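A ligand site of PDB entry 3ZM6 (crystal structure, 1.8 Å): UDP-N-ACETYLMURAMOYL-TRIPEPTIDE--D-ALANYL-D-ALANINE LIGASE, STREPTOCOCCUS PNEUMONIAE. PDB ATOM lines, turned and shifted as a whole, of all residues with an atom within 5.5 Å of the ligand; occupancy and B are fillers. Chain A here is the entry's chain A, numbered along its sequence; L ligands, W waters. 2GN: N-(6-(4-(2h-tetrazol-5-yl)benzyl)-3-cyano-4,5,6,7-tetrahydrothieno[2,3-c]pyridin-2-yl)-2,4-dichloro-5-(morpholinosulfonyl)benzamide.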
ATOM      1  N   PHE A  31      -6.319  -0.566 -20.885  1.00  0.00           N
ATOM      2  CA  PHE A  31      -6.353  -2.051 -20.865  1.00  0.00           C
ATOM      3  C   PHE A  31      -7.757  -2.610 -21.108  1.00  0.00           C
ATOM      4  O   PHE A  31      -7.903  -3.831 -21.302  1.00  0.00           O
ATOM      5  CB  PHE A  31      -5.753  -2.619 -19.555  1.00  0.00           C
ATOM      6  CG  PHE A  31      -6.337  -1.996 -18.282  1.00  0.00           C
ATOM      7  CD1 PHE A  31      -7.623  -2.305 -17.882  1.00  0.00           C
ATOM      8  CD2 PHE A  31      -5.585  -1.140 -17.471  1.00  0.00           C
ATOM      9  CE1 PHE A  31      -8.171  -1.765 -16.704  1.00  0.00           C
ATOM     10  CE2 PHE A  31      -6.132  -0.598 -16.302  1.00  0.00           C
ATOM     11  CZ  PHE A  31      -7.421  -0.895 -15.909  1.00  0.00           C
ATOM     12  N   ASP A  32      -8.739  -1.712 -21.069  1.00  0.00           N
ATOM     13  CA  ASP A  32     -10.165  -1.948 -21.304  1.00  0.00           C
ATOM     14  C   ASP A  32     -10.463  -1.422 -22.708  1.00  0.00           C
ATOM     15  O   ASP A  32     -10.414  -0.193 -22.957  1.00  0.00           O
ATOM     16  CB  ASP A  32     -10.987  -1.095 -20.317  1.00  0.00           C
ATOM     17  CG  ASP A  32     -12.521  -1.290 -20.455  1.00  0.00           C
ATOM     18  OD1 ASP A  32     -13.021  -1.729 -21.535  1.00  0.00           O
ATOM     19  OD2 ASP A  32     -13.250  -0.969 -19.447  1.00  0.00           O
ATOM     20  N   SER A  33     -10.741  -2.326 -23.656  1.00  0.00           N
ATOM     21  CA  SER A  33     -10.838  -1.892 -25.029  1.00  0.00           C
ATOM     22  C   SER A  33     -12.018  -0.921 -25.245  1.00  0.00           C
ATOM     23  O   SER A  33     -12.028  -0.157 -26.205  1.00  0.00           O
ATOM     24  CB  SER A  33     -10.985  -3.099 -25.971  1.00  0.00           C
ATOM     25  OG  SER A  33     -12.218  -3.762 -25.751  1.00  0.00           O
ATOM     26  N   ARG A  34     -13.014  -0.955 -24.368  1.00  0.00           N
ATOM     27  CA  ARG A  34     -14.138  -0.025 -24.508  1.00  0.00           C
ATOM     28  C   ARG A  34     -13.664   1.412 -24.416  1.00  0.00           C
ATOM     29  O   ARG A  34     -14.363   2.326 -24.852  1.00  0.00           O
ATOM     30  CB  ARG A  34     -15.176  -0.250 -23.429  1.00  0.00           C
ATOM     31  CG  ARG A  34     -15.823  -1.631 -23.455  1.00  0.00           C
ATOM     32  CD  ARG A  34     -16.759  -1.774 -22.272  1.00  0.00           C
ATOM     33  NE  ARG A  34     -15.972  -1.900 -21.041  1.00  0.00           N
ATOM     34  CZ  ARG A  34     -16.511  -2.179 -19.867  1.00  0.00           C
ATOM     35  NH1 ARG A  34     -17.841  -2.374 -19.760  1.00  0.00           N
ATOM     36  NH2 ARG A  34     -15.722  -2.261 -18.800  1.00  0.00           N
ATOM     37  N   LEU A  45      -3.819  -7.049 -20.672  1.00  0.00           N
ATOM     38  CA  LEU A  45      -3.390  -7.578 -19.395  1.00  0.00           C
ATOM     39  C   LEU A  45      -4.099  -8.896 -19.074  1.00  0.00           C
ATOM     40  O   LEU A  45      -5.064  -9.260 -19.760  1.00  0.00           O
ATOM     41  CB  LEU A  45      -3.632  -6.541 -18.281  1.00  0.00           C
ATOM     42  CG  LEU A  45      -2.905  -5.200 -18.447  1.00  0.00           C
ATOM     43  CD1 LEU A  45      -3.416  -4.186 -17.412  1.00  0.00           C
ATOM     44  CD2 LEU A  45      -1.372  -5.334 -18.415  1.00  0.00           C
ATOM     45  N   LYS A  46      -3.615  -9.621 -18.068  1.00  0.00           N
ATOM     46  CA  LYS A  46      -4.320 -10.868 -17.674  1.00  0.00           C
ATOM     47  C   LYS A  46      -5.509 -10.489 -16.808  1.00  0.00           C
ATOM     48  O   LYS A  46      -5.363 -10.345 -15.620  1.00  0.00           O
ATOM     49  CB  LYS A  46      -3.406 -11.855 -16.909  1.00  0.00           C
ATOM     50  CG  LYS A  46      -2.198 -12.396 -17.674  1.00  0.00           C
ATOM     51  CD  LYS A  46      -1.569 -13.609 -16.964  1.00  0.00           C
ATOM     52  CE  LYS A  46      -0.058 -13.696 -17.149  1.00  0.00           C
ATOM     53  NZ  LYS A  46       0.443 -13.819 -18.555  1.00  0.00           N
ATOM     54  N   GLY A  47      -6.684 -10.317 -17.409  1.00  0.00           N
ATOM     55  CA  GLY A  47      -7.879  -9.947 -16.609  1.00  0.00           C
ATOM     56  C   GLY A  47      -8.757 -11.173 -16.441  1.00  0.00           C
ATOM     57  O   GLY A  47      -8.276 -12.282 -16.327  1.00  0.00           O
ATOM     58  N   ALA A  48     -10.072 -10.989 -16.402  1.00  0.00           N
ATOM     59  CA  ALA A  48     -10.972 -12.168 -16.451  1.00  0.00           C
ATOM     60  C   ALA A  48     -10.713 -12.989 -17.732  1.00  0.00           C
ATOM     61  O   ALA A  48     -10.736 -14.220 -17.690  1.00  0.00           O
ATOM     62  CB  ALA A  48     -12.415 -11.716 -16.366  1.00  0.00           C
ATOM     63  N   ARG A  49     -10.491 -12.310 -18.855  1.00  0.00           N
ATOM     64  CA  ARG A  49      -9.842 -12.900 -20.020  1.00  0.00           C
ATOM     65  C   ARG A  49      -8.502 -12.204 -20.243  1.00  0.00           C
ATOM     66  O   ARG A  49      -8.298 -11.048 -19.875  1.00  0.00           O
ATOM     67  CB  ARG A  49     -10.651 -12.710 -21.318  1.00  0.00           C
ATOM     68  CG  ARG A  49     -12.122 -13.048 -21.273  1.00  0.00           C
ATOM     69  CD  ARG A  49     -12.450 -14.391 -21.891  1.00  0.00           C
ATOM     70  NE  ARG A  49     -11.800 -14.755 -23.157  1.00  0.00           N
ATOM     71  CZ  ARG A  49     -12.068 -15.905 -23.778  1.00  0.00           C
ATOM     72  NH1 ARG A  49     -12.923 -16.732 -23.223  1.00  0.00           N
ATOM     73  NH2 ARG A  49     -11.469 -16.276 -24.925  1.00  0.00           N
ATOM     74  N   ASP A  50      -7.585 -12.898 -20.875  1.00  0.00           N
ATOM     75  CA  ASP A  50      -6.349 -12.257 -21.309  1.00  0.00           C
ATOM     76  C   ASP A  50      -6.656 -11.157 -22.320  1.00  0.00           C
ATOM     77  O   ASP A  50      -7.304 -11.431 -23.333  1.00  0.00           O
ATOM     78  CB  ASP A  50      -5.450 -13.296 -21.927  1.00  0.00           C
ATOM     79  CG  ASP A  50      -4.065 -12.770 -22.237  1.00  0.00           C
ATOM     80  OD1 ASP A  50      -3.941 -11.657 -22.785  1.00  0.00           O
ATOM     81  OD2 ASP A  50      -3.112 -13.492 -21.925  1.00  0.00           O
ATOM     82  N   PHE A  54      -8.535  -9.209 -27.031  1.00  0.00           N
ATOM     83  CA  PHE A  54      -9.324  -8.013 -27.414  1.00  0.00           C
ATOM     84  C   PHE A  54      -8.522  -7.028 -28.240  1.00  0.00           C
ATOM     85  O   PHE A  54      -8.939  -5.865 -28.459  1.00  0.00           O
ATOM     86  CB  PHE A  54      -9.898  -7.348 -26.160  1.00  0.00           C
ATOM     87  CG  PHE A  54     -10.663  -8.307 -25.292  1.00  0.00           C
ATOM     88  CD1 PHE A  54     -11.865  -8.872 -25.751  1.00  0.00           C
ATOM     89  CD2 PHE A  54     -10.164  -8.706 -24.066  1.00  0.00           C
ATOM     90  CE1 PHE A  54     -12.563  -9.774 -24.955  1.00  0.00           C
ATOM     91  CE2 PHE A  54     -10.862  -9.608 -23.270  1.00  0.00           C
ATOM     92  CZ  PHE A  54     -12.057 -10.138 -23.719  1.00  0.00           C
ATOM     93  N   THR A  57     -10.455  -5.818 -31.373  1.00  0.00           N
ATOM     94  CA  THR A  57     -11.436  -4.823 -30.931  1.00  0.00           C
ATOM     95  C   THR A  57     -10.781  -3.455 -30.625  1.00  0.00           C
ATOM     96  O   THR A  57     -11.310  -2.391 -30.985  1.00  0.00           O
ATOM     97  CB  THR A  57     -12.227  -5.347 -29.721  1.00  0.00           C
ATOM     98  OG1 THR A  57     -12.861  -6.588 -30.102  1.00  0.00           O
ATOM     99  CG2 THR A  57     -13.301  -4.348 -29.315  1.00  0.00           C
ATOM    100  N   GLU A  60     -10.099  -1.906 -33.927  1.00  0.00           N
ATOM    101  CA  GLU A  60     -11.391  -1.441 -34.473  1.00  0.00           C
ATOM    102  C   GLU A  60     -11.775  -0.126 -33.801  1.00  0.00           C
ATOM    103  O   GLU A  60     -12.343   0.737 -34.440  1.00  0.00           O
ATOM    104  CB  GLU A  60     -12.511  -2.449 -34.240  1.00  0.00           C
ATOM    105  CG  GLU A  60     -12.424  -3.700 -35.072  1.00  0.00           C
ATOM    106  CD  GLU A  60     -13.376  -4.797 -34.570  1.00  0.00           C
ATOM    107  OE1 GLU A  60     -14.130  -4.606 -33.580  1.00  0.00           O
ATOM    108  OE2 GLU A  60     -13.339  -5.891 -35.142  1.00  0.00           O
ATOM    109  N   ASN A 134     -10.184   3.358  -6.936  1.00  0.00           N
ATOM    110  CA  ASN A 134      -9.257   2.449  -6.283  1.00  0.00           C
ATOM    111  C   ASN A 134      -8.124   1.908  -7.168  1.00  0.00           C
ATOM    112  O   ASN A 134      -7.715   0.770  -7.016  1.00  0.00           O
ATOM    113  CB  ASN A 134     -10.031   1.286  -5.673  1.00  0.00           C
ATOM    114  CG  ASN A 134     -10.649   0.373  -6.699  1.00  0.00           C
ATOM    115  OD1 ASN A 134     -10.503   0.567  -7.916  1.00  0.00           O
ATOM    116  ND2 ASN A 134     -11.357  -0.638  -6.228  1.00  0.00           N
ATOM    117  N   TYR A 135      -7.614   2.730  -8.084  1.00  0.00           N
ATOM    118  CA  TYR A 135      -6.564   2.339  -8.994  1.00  0.00           C
ATOM    119  C   TYR A 135      -5.211   2.409  -8.312  1.00  0.00           C
ATOM    120  O   TYR A 135      -4.348   3.149  -8.734  1.00  0.00           O
ATOM    121  CB  TYR A 135      -6.585   3.234 -10.220  1.00  0.00           C
ATOM    122  CG  TYR A 135      -7.471   2.657 -11.338  1.00  0.00           C
ATOM    123  CD1 TYR A 135      -8.766   2.238 -11.084  1.00  0.00           C
ATOM    124  CD2 TYR A 135      -7.003   2.608 -12.652  1.00  0.00           C
ATOM    125  CE1 TYR A 135      -9.574   1.705 -12.120  1.00  0.00           C
ATOM    126  CE2 TYR A 135      -7.794   2.113 -13.676  1.00  0.00           C
ATOM    127  CZ  TYR A 135      -9.054   1.650 -13.412  1.00  0.00           C
ATOM    128  OH  TYR A 135      -9.805   1.182 -14.477  1.00  0.00           O
ATOM    129  N   ASN A 136      -5.048   1.628  -7.262  1.00  0.00           N
ATOM    130  CA  ASN A 136      -3.936   1.791  -6.330  1.00  0.00           C
ATOM    131  C   ASN A 136      -2.953   0.591  -6.361  1.00  0.00           C
ATOM    132  O   ASN A 136      -2.107   0.461  -5.450  1.00  0.00           O
ATOM    133  CB  ASN A 136      -4.490   2.018  -4.898  1.00  0.00           C
ATOM    134  CG  ASN A 136      -5.216   0.815  -4.358  1.00  0.00           C
ATOM    135  OD1 ASN A 136      -5.139  -0.277  -4.915  1.00  0.00           O
ATOM    136  ND2 ASN A 136      -6.016   1.016  -3.305  1.00  0.00           N
ATOM    137  N   ASN A 137      -3.080  -0.300  -7.336  1.00  0.00           N
ATOM    138  CA  ASN A 137      -2.281  -1.542  -7.278  1.00  0.00           C
ATOM    139  C   ASN A 137      -1.306  -1.632  -8.442  1.00  0.00           C
ATOM    140  O   ASN A 137      -1.037  -0.632  -9.095  1.00  0.00           O
ATOM    141  CB  ASN A 137      -3.172  -2.778  -7.135  1.00  0.00           C
ATOM    142  CG  ASN A 137      -3.911  -3.138  -8.430  1.00  0.00           C
ATOM    143  OD1 ASN A 137      -3.886  -2.411  -9.450  1.00  0.00           O
ATOM    144  ND2 ASN A 137      -4.618  -4.241  -8.381  1.00  0.00           N
ATOM    145  N   ILE A 139      -1.458  -2.575 -11.289  1.00  0.00           N
ATOM    146  CA  ILE A 139      -2.069  -2.197 -12.571  1.00  0.00           C
ATOM    147  C   ILE A 139      -2.639  -0.765 -12.484  1.00  0.00           C
ATOM    148  O   ILE A 139      -2.375   0.090 -13.356  1.00  0.00           O
ATOM    149  CB  ILE A 139      -3.182  -3.201 -12.993  1.00  0.00           C
ATOM    150  CG1 ILE A 139      -2.582  -4.589 -13.337  1.00  0.00           C
ATOM    151  CG2 ILE A 139      -4.047  -2.646 -14.118  1.00  0.00           C
ATOM    152  CD1 ILE A 139      -3.615  -5.599 -13.827  1.00  0.00           C
ATOM    153  N   GLY A 140      -3.408  -0.472 -11.435  1.00  0.00           N
ATOM    154  CA  GLY A 140      -4.026   0.863 -11.306  1.00  0.00           C
ATOM    155  C   GLY A 140      -3.029   2.011 -11.196  1.00  0.00           C
ATOM    156  O   GLY A 140      -3.241   3.100 -11.754  1.00  0.00           O
ATOM    157  N   ASN A 326     -15.736  -0.354  -9.973  1.00  0.00           N
ATOM    158  CA  ASN A 326     -15.267  -1.131 -11.131  1.00  0.00           C
ATOM    159  C   ASN A 326     -16.231  -2.220 -11.546  1.00  0.00           C
ATOM    160  O   ASN A 326     -16.105  -3.381 -11.150  1.00  0.00           O
ATOM    161  CB  ASN A 326     -13.878  -1.744 -10.892  1.00  0.00           C
ATOM    162  CG  ASN A 326     -12.856  -0.723 -10.420  1.00  0.00           C
ATOM    163  OD1 ASN A 326     -12.660   0.318 -11.045  1.00  0.00           O
ATOM    164  ND2 ASN A 326     -12.192  -1.011  -9.317  1.00  0.00           N
ATOM    165  N   ASN A 328     -16.617  -4.276 -13.895  1.00  0.00           N
ATOM    166  CA  ASN A 328     -16.082  -5.024 -15.061  1.00  0.00           C
ATOM    167  C   ASN A 328     -15.748  -6.452 -14.674  1.00  0.00           C
ATOM    168  O   ASN A 328     -15.683  -6.795 -13.495  1.00  0.00           O
ATOM    169  CB  ASN A 328     -14.878  -4.290 -15.690  1.00  0.00           C
ATOM    170  CG  ASN A 328     -13.652  -4.324 -14.807  1.00  0.00           C
ATOM    171  OD1 ASN A 328     -13.067  -5.387 -14.578  1.00  0.00           O
ATOM    172  ND2 ASN A 328     -13.319  -3.179 -14.235  1.00  0.00           N
ATOM    173  N   PRO A 329     -15.576  -7.325 -15.673  1.00  0.00           N
ATOM    174  CA  PRO A 329     -15.420  -8.729 -15.366  1.00  0.00           C
ATOM    175  C   PRO A 329     -14.183  -9.085 -14.553  1.00  0.00           C
ATOM    176  O   PRO A 329     -14.222 -10.049 -13.758  1.00  0.00           O
ATOM    177  CB  PRO A 329     -15.361  -9.389 -16.771  1.00  0.00           C
ATOM    178  CG  PRO A 329     -16.020  -8.382 -17.678  1.00  0.00           C
ATOM    179  CD  PRO A 329     -15.526  -7.078 -17.121  1.00  0.00           C
ATOM    180  N   THR A 330     -13.081  -8.382 -14.791  1.00  0.00           N
ATOM    181  CA  THR A 330     -11.851  -8.607 -14.025  1.00  0.00           C
ATOM    182  C   THR A 330     -12.064  -8.238 -12.558  1.00  0.00           C
ATOM    183  O   THR A 330     -11.704  -9.005 -11.677  1.00  0.00           O
ATOM    184  CB  THR A 330     -10.671  -7.815 -14.576  1.00  0.00           C
ATOM    185  OG1 THR A 330     -10.515  -8.093 -15.969  1.00  0.00           O
ATOM    186  CG2 THR A 330      -9.345  -8.157 -13.805  1.00  0.00           C
ATOM    187  N   ALA A 331     -12.673  -7.074 -12.311  1.00  0.00           N
ATOM    188  CA  ALA A 331     -13.006  -6.687 -10.931  1.00  0.00           C
ATOM    189  C   ALA A 331     -13.907  -7.738 -10.266  1.00  0.00           C
ATOM    190  O   ALA A 331     -13.768  -8.020  -9.075  1.00  0.00           O
ATOM    191  CB  ALA A 331     -13.602  -5.292 -10.867  1.00  0.00           C
ATOM    192  N   LEU A 334     -11.706 -10.691  -9.481  1.00  0.00           N
ATOM    193  CA  LEU A 334     -10.720 -10.404  -8.460  1.00  0.00           C
ATOM    194  C   LEU A 334     -11.345 -10.370  -7.078  1.00  0.00           C
ATOM    195  O   LEU A 334     -10.757 -10.837  -6.094  1.00  0.00           O
ATOM    196  CB  LEU A 334     -10.029  -9.079  -8.749  1.00  0.00           C
ATOM    197  CG  LEU A 334      -8.984  -9.117  -9.871  1.00  0.00           C
ATOM    198  CD1 LEU A 334      -8.353  -7.749 -10.037  1.00  0.00           C
ATOM    199  CD2 LEU A 334      -7.931 -10.167  -9.511  1.00  0.00           C
ATOM    200  N   GLU A 359     -22.823  -3.041 -20.110  1.00  0.00           N
ATOM    201  CA  GLU A 359     -22.010  -2.513 -21.213  1.00  0.00           C
ATOM    202  C   GLU A 359     -20.888  -3.452 -21.650  1.00  0.00           C
ATOM    203  O   GLU A 359     -19.764  -3.022 -21.871  1.00  0.00           O
ATOM    204  CB  GLU A 359     -21.493  -1.089 -20.913  1.00  0.00           C
ATOM    205  CG  GLU A 359     -21.728  -0.607 -19.488  1.00  0.00           C
ATOM    206  CD  GLU A 359     -22.664   0.589 -19.412  1.00  0.00           C
ATOM    207  OE1 GLU A 359     -22.263   1.677 -19.894  1.00  0.00           O
ATOM    208  OE2 GLU A 359     -23.793   0.483 -18.858  1.00  0.00           O
ATOM    209  N   LEU A 360     -21.198  -4.742 -21.750  1.00  0.00           N
ATOM    210  CA  LEU A 360     -20.236  -5.701 -22.278  1.00  0.00           C
ATOM    211  C   LEU A 360     -20.621  -6.047 -23.709  1.00  0.00           C
ATOM    212  O   LEU A 360     -20.042  -6.954 -24.312  1.00  0.00           O
ATOM    213  CB  LEU A 360     -20.214  -6.962 -21.397  1.00  0.00           C
ATOM    214  CG  LEU A 360     -19.710  -6.696 -19.980  1.00  0.00           C
ATOM    215  CD1 LEU A 360     -19.743  -7.952 -19.164  1.00  0.00           C
ATOM    216  CD2 LEU A 360     -18.292  -6.138 -20.059  1.00  0.00           C
ATOM    217  N   GLY A 361     -21.614  -5.323 -24.221  1.00  0.00           N
ATOM    218  CA  GLY A 361     -22.045  -5.444 -25.612  1.00  0.00           C
ATOM    219  C   GLY A 361     -22.427  -6.853 -25.971  1.00  0.00           C
ATOM    220  O   GLY A 361     -23.095  -7.558 -25.201  1.00  0.00           O
ATOM    221  N   ASP A 362     -21.962  -7.262 -27.139  1.00  0.00           N
ATOM    222  CA  ASP A 362     -22.250  -8.567 -27.753  1.00  0.00           C
ATOM    223  C   ASP A 362     -21.610  -9.713 -26.940  1.00  0.00           C
ATOM    224  O   ASP A 362     -22.040 -10.838 -27.012  1.00  0.00           O
ATOM    225  CB  ASP A 362     -21.700  -8.624 -29.210  1.00  0.00           C
ATOM    226  CG  ASP A 362     -22.596  -7.882 -30.242  1.00  0.00           C
ATOM    227  OD1 ASP A 362     -23.825  -8.081 -30.264  1.00  0.00           O
ATOM    228  OD2 ASP A 362     -22.024  -7.141 -31.093  1.00  0.00           O
ATOM    229  N   GLN A 363     -20.579  -9.401 -26.159  1.00  0.00           N
ATOM    230  CA  GLN A 363     -19.847 -10.419 -25.396  1.00  0.00           C
ATOM    231  C   GLN A 363     -20.378 -10.671 -23.963  1.00  0.00           C
ATOM    232  O   GLN A 363     -19.758 -11.411 -23.202  1.00  0.00           O
ATOM    233  CB  GLN A 363     -18.366  -9.990 -25.258  1.00  0.00           C
ATOM    234  CG  GLN A 363     -17.514 -10.085 -26.515  1.00  0.00           C
ATOM    235  CD  GLN A 363     -16.682 -11.362 -26.570  1.00  0.00           C
ATOM    236  OE1 GLN A 363     -16.763 -12.110 -27.551  1.00  0.00           O
ATOM    237  NE2 GLN A 363     -15.866 -11.631 -25.512  1.00  0.00           N
ATOM    238  N   LEU A 367     -18.771 -13.450 -20.992  1.00  0.00           N
ATOM    239  CA  LEU A 367     -17.878 -12.918 -19.949  1.00  0.00           C
ATOM    240  C   LEU A 367     -18.432 -13.218 -18.585  1.00  0.00           C
ATOM    241  O   LEU A 367     -17.685 -13.368 -17.624  1.00  0.00           O
ATOM    242  CB  LEU A 367     -17.656 -11.412 -20.096  1.00  0.00           C
ATOM    243  CG  LEU A 367     -16.855 -10.982 -21.353  1.00  0.00           C
ATOM    244  CD1 LEU A 367     -17.125  -9.542 -21.815  1.00  0.00           C
ATOM    245  CD2 LEU A 367     -15.379 -11.265 -21.179  1.00  0.00           C
HETATM  246  O25 2GN L   1     -10.909  -3.029 -12.262  1.00  0.00           O
HETATM  247  S21 2GN L   1      -9.730  -3.811 -12.003  1.00  0.00           S
HETATM  248  O24 2GN L   1      -9.938  -4.814 -11.023  1.00  0.00           O
HETATM  249  N23 2GN L   1      -8.534  -2.757 -11.425  1.00  0.00           N
HETATM  250  C28 2GN L   1      -8.401  -2.708  -9.972  1.00  0.00           C
HETATM  251  C30 2GN L   1      -6.983  -2.195  -9.835  1.00  0.00           C
HETATM  252  O31 2GN L   1      -6.871  -0.905 -10.438  1.00  0.00           O
HETATM  253  C29 2GN L   1      -7.093  -0.968 -11.849  1.00  0.00           C
HETATM  254  C27 2GN L   1      -8.528  -1.473 -12.089  1.00  0.00           C
HETATM  255  C18 2GN L   1      -9.177  -4.397 -13.423  1.00  0.00           C
HETATM  256  C16 2GN L   1      -9.991  -4.259 -14.528  1.00  0.00           C
HETATM  257  C22 2GN L   1      -7.903  -4.983 -13.560  1.00  0.00           C
HETATM  258 CL2  2GN L   1      -6.763  -5.231 -12.243  1.00  0.00          CL
HETATM  259  C19 2GN L   1      -7.481  -5.450 -14.789  1.00  0.00           C
HETATM  260  C17 2GN L   1      -8.303  -5.351 -15.885  1.00  0.00           C
HETATM  261 CL1  2GN L   1      -7.671  -5.972 -17.435  1.00  0.00          CL
HETATM  262  C14 2GN L   1      -9.551  -4.738 -15.770  1.00  0.00           C
HETATM  263  C13 2GN L   1     -10.509  -4.644 -16.888  1.00  0.00           C
HETATM  264  O15 2GN L   1     -11.094  -3.600 -17.132  1.00  0.00           O
HETATM  265  N10 2GN L   1     -10.793  -5.897 -17.571  1.00  0.00           N
HETATM  266  C5  2GN L   1     -11.673  -5.883 -18.601  1.00  0.00           C
HETATM  267  C2  2GN L   1     -12.048  -6.999 -19.356  1.00  0.00           C
HETATM  268  C6  2GN L   1     -11.509  -8.277 -19.098  1.00  0.00           C
HETATM  269  N11 2GN L   1     -11.101  -9.339 -18.851  1.00  0.00           N
HETATM  270  S7  2GN L   1     -12.546  -4.522 -19.152  1.00  0.00           S
HETATM  271  C3  2GN L   1     -13.361  -5.416 -20.438  1.00  0.00           C
HETATM  272  C8  2GN L   1     -14.314  -4.684 -21.310  1.00  0.00           C
HETATM  273  N12 2GN L   1     -14.726  -5.579 -22.379  1.00  0.00           N
HETATM  274  C9  2GN L   1     -14.262  -6.960 -22.574  1.00  0.00           C
HETATM  275  C4  2GN L   1     -13.608  -7.721 -21.419  1.00  0.00           C
HETATM  276  C1  2GN L   1     -13.037  -6.751 -20.432  1.00  0.00           C
HETATM  277  C32 2GN L   1     -15.665  -5.002 -23.315  1.00  0.00           C
HETATM  278  C33 2GN L   1     -15.720  -5.700 -24.667  1.00  0.00           C
HETATM  279  C38 2GN L   1     -14.575  -6.188 -25.306  1.00  0.00           C
HETATM  280  C37 2GN L   1     -14.679  -6.836 -26.543  1.00  0.00           C
HETATM  281  C36 2GN L   1     -15.949  -6.975 -27.124  1.00  0.00           C
HETATM  282  C35 2GN L   1     -17.098  -6.478 -26.483  1.00  0.00           C
HETATM  283  C34 2GN L   1     -16.973  -5.854 -25.251  1.00  0.00           C
HETATM  284  C06 2GN L   1     -16.122  -7.664 -28.440  1.00  0.00           C
HETATM  285  N01 2GN L   1     -15.481  -8.794 -28.811  1.00  0.00           N
HETATM  286  N02 2GN L   1     -16.980  -7.285 -29.427  1.00  0.00           N
HETATM  287  N05 2GN L   1     -16.871  -8.192 -30.482  1.00  0.00           N
HETATM  288  N04 2GN L   1     -15.919  -9.156 -30.094  1.00  0.00           N
HETATM  289  O   HOH W   1     -11.844  -4.972 -23.380  1.00  0.00           O
HETATM  290  O   HOH W   2     -11.422  -3.770  -8.591  1.00  0.00           O
HETATM  291  O   HOH W   3     -11.904  -1.034 -16.998  1.00  0.00           O
HETATM  292  O   HOH W   4      -8.367  -8.207 -20.276  1.00  0.00           O
HETATM  293  O   HOH W   5      -4.938  -6.777 -10.050  1.00  0.00           O
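OD1 of Asn 137 sits close to O31 of the ligand (3.5 Å). N of Arg 49 sits at hydrogen-bond distance from N11 of the ligand (3.0 Å). The side-chain amide nitrogen of Asn 328 sits at hydrogen-bond distance from an oxygen (O25) of the ligand. The side-chain hydroxyl (OG1) of Thr 330 lies within hydrogen-bond range of a nitrogen (N10) of the ligand. N11 of the ligand lies within hydrogen-bond range of N of Ala 48 (3.1 Å).
The backbone NH of Thr 330 is in hydrogen-bond range of the side-chain amide oxygen of Asn 328 (3.0 Å). The side-chain amide oxygen (OD1) of Asn 137 lies within hydrogen-bond range of the backbone NH (N) of Gly 140, at 2.8 Å. OD1 of Asn 137 lies close to N of Ile 139 (3.1 Å). OG1 of Thr 330 sits at hydrogen-bond distance from N of Ala 48 (3.0 Å). The side-chain carboxylate (OD2) of Asp 32 is in salt-bridge range of the guanidinium group (NH2) of Arg 34 (2.9 Å). The backbone carbonyl oxygen (O) of Glu 359 sits at hydrogen-bond distance from the guanidinium group (NH1) of Arg 34, 2.9 Å away. The backbone carbonyl oxygen (O) of Asn 134 sits close to the side-chain amide oxygen (OD1) of Asn 136, at 3.5 Å. ND2 of Asn 326 is in hydrogen-bond range of OD1 of Asn 134 (2.7 Å).
OD2 of Asp 32 sits close to S7 of the ligand, at 3.6 Å. Phe 31 touches the ligand. Ser 33 touches the ligand. Arg 34 touches the ligand. Gly 47 touches the ligand. Phe 54 touches the ligand. Thr 57 touches the ligand. Asn 134 touches the ligand. Tyr 135 touches the ligand (CE1 to C27, 3.3 Å). Ile 139 touches the ligand. Gly 140 touches the ligand (CA to O31, 3.5 Å). Asn 326 touches the ligand. CA of Ala 331 touches O24 of the ligand, at 3.6 Å. CD1 of Leu 334 touches O24 of the ligand, 3.5 Å away. Leu 360 touches the ligand. Gln 363 touches the ligand. CD1 of Leu 367 touches C9 of the ligand (3.9 Å). Hydrophobic or aromatic side chains within 4 Å of the ligand: Phe 31, Ala 48, Phe 54, Tyr 135, Ile 139, Ala 331, Leu 334 and Leu 367. Within 4 Å of the ligand: Phe 31, Asp 32, Ser 33, Arg 34, Gly 47, Ala 48, Arg 49, Phe 54, Thr 57, Asn 134, Tyr 135, Asn 137, Ile 139, Gly 140, Asn 326, Asn 328, Thr 330, Ala 331, Leu 334, Leu 360, Gln 363 and Leu 367. Along chain A the residues within 4 Å of the ligand span positions 31 to 367.
Water W3 lies within hydrogen-bond range of an oxygen (O15) of the ligand (2.7 Å) and the side-chain carboxylate (OD2) of Asp 32 (2.8 Å). Water W2 bridges ND2 of Asn 326 (3.0 Å) and O24 of the ligand (3.0 Å). Water W4 bridges O of Arg 49 (2.9 Å) and N11 of the ligand (3.3 Å).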
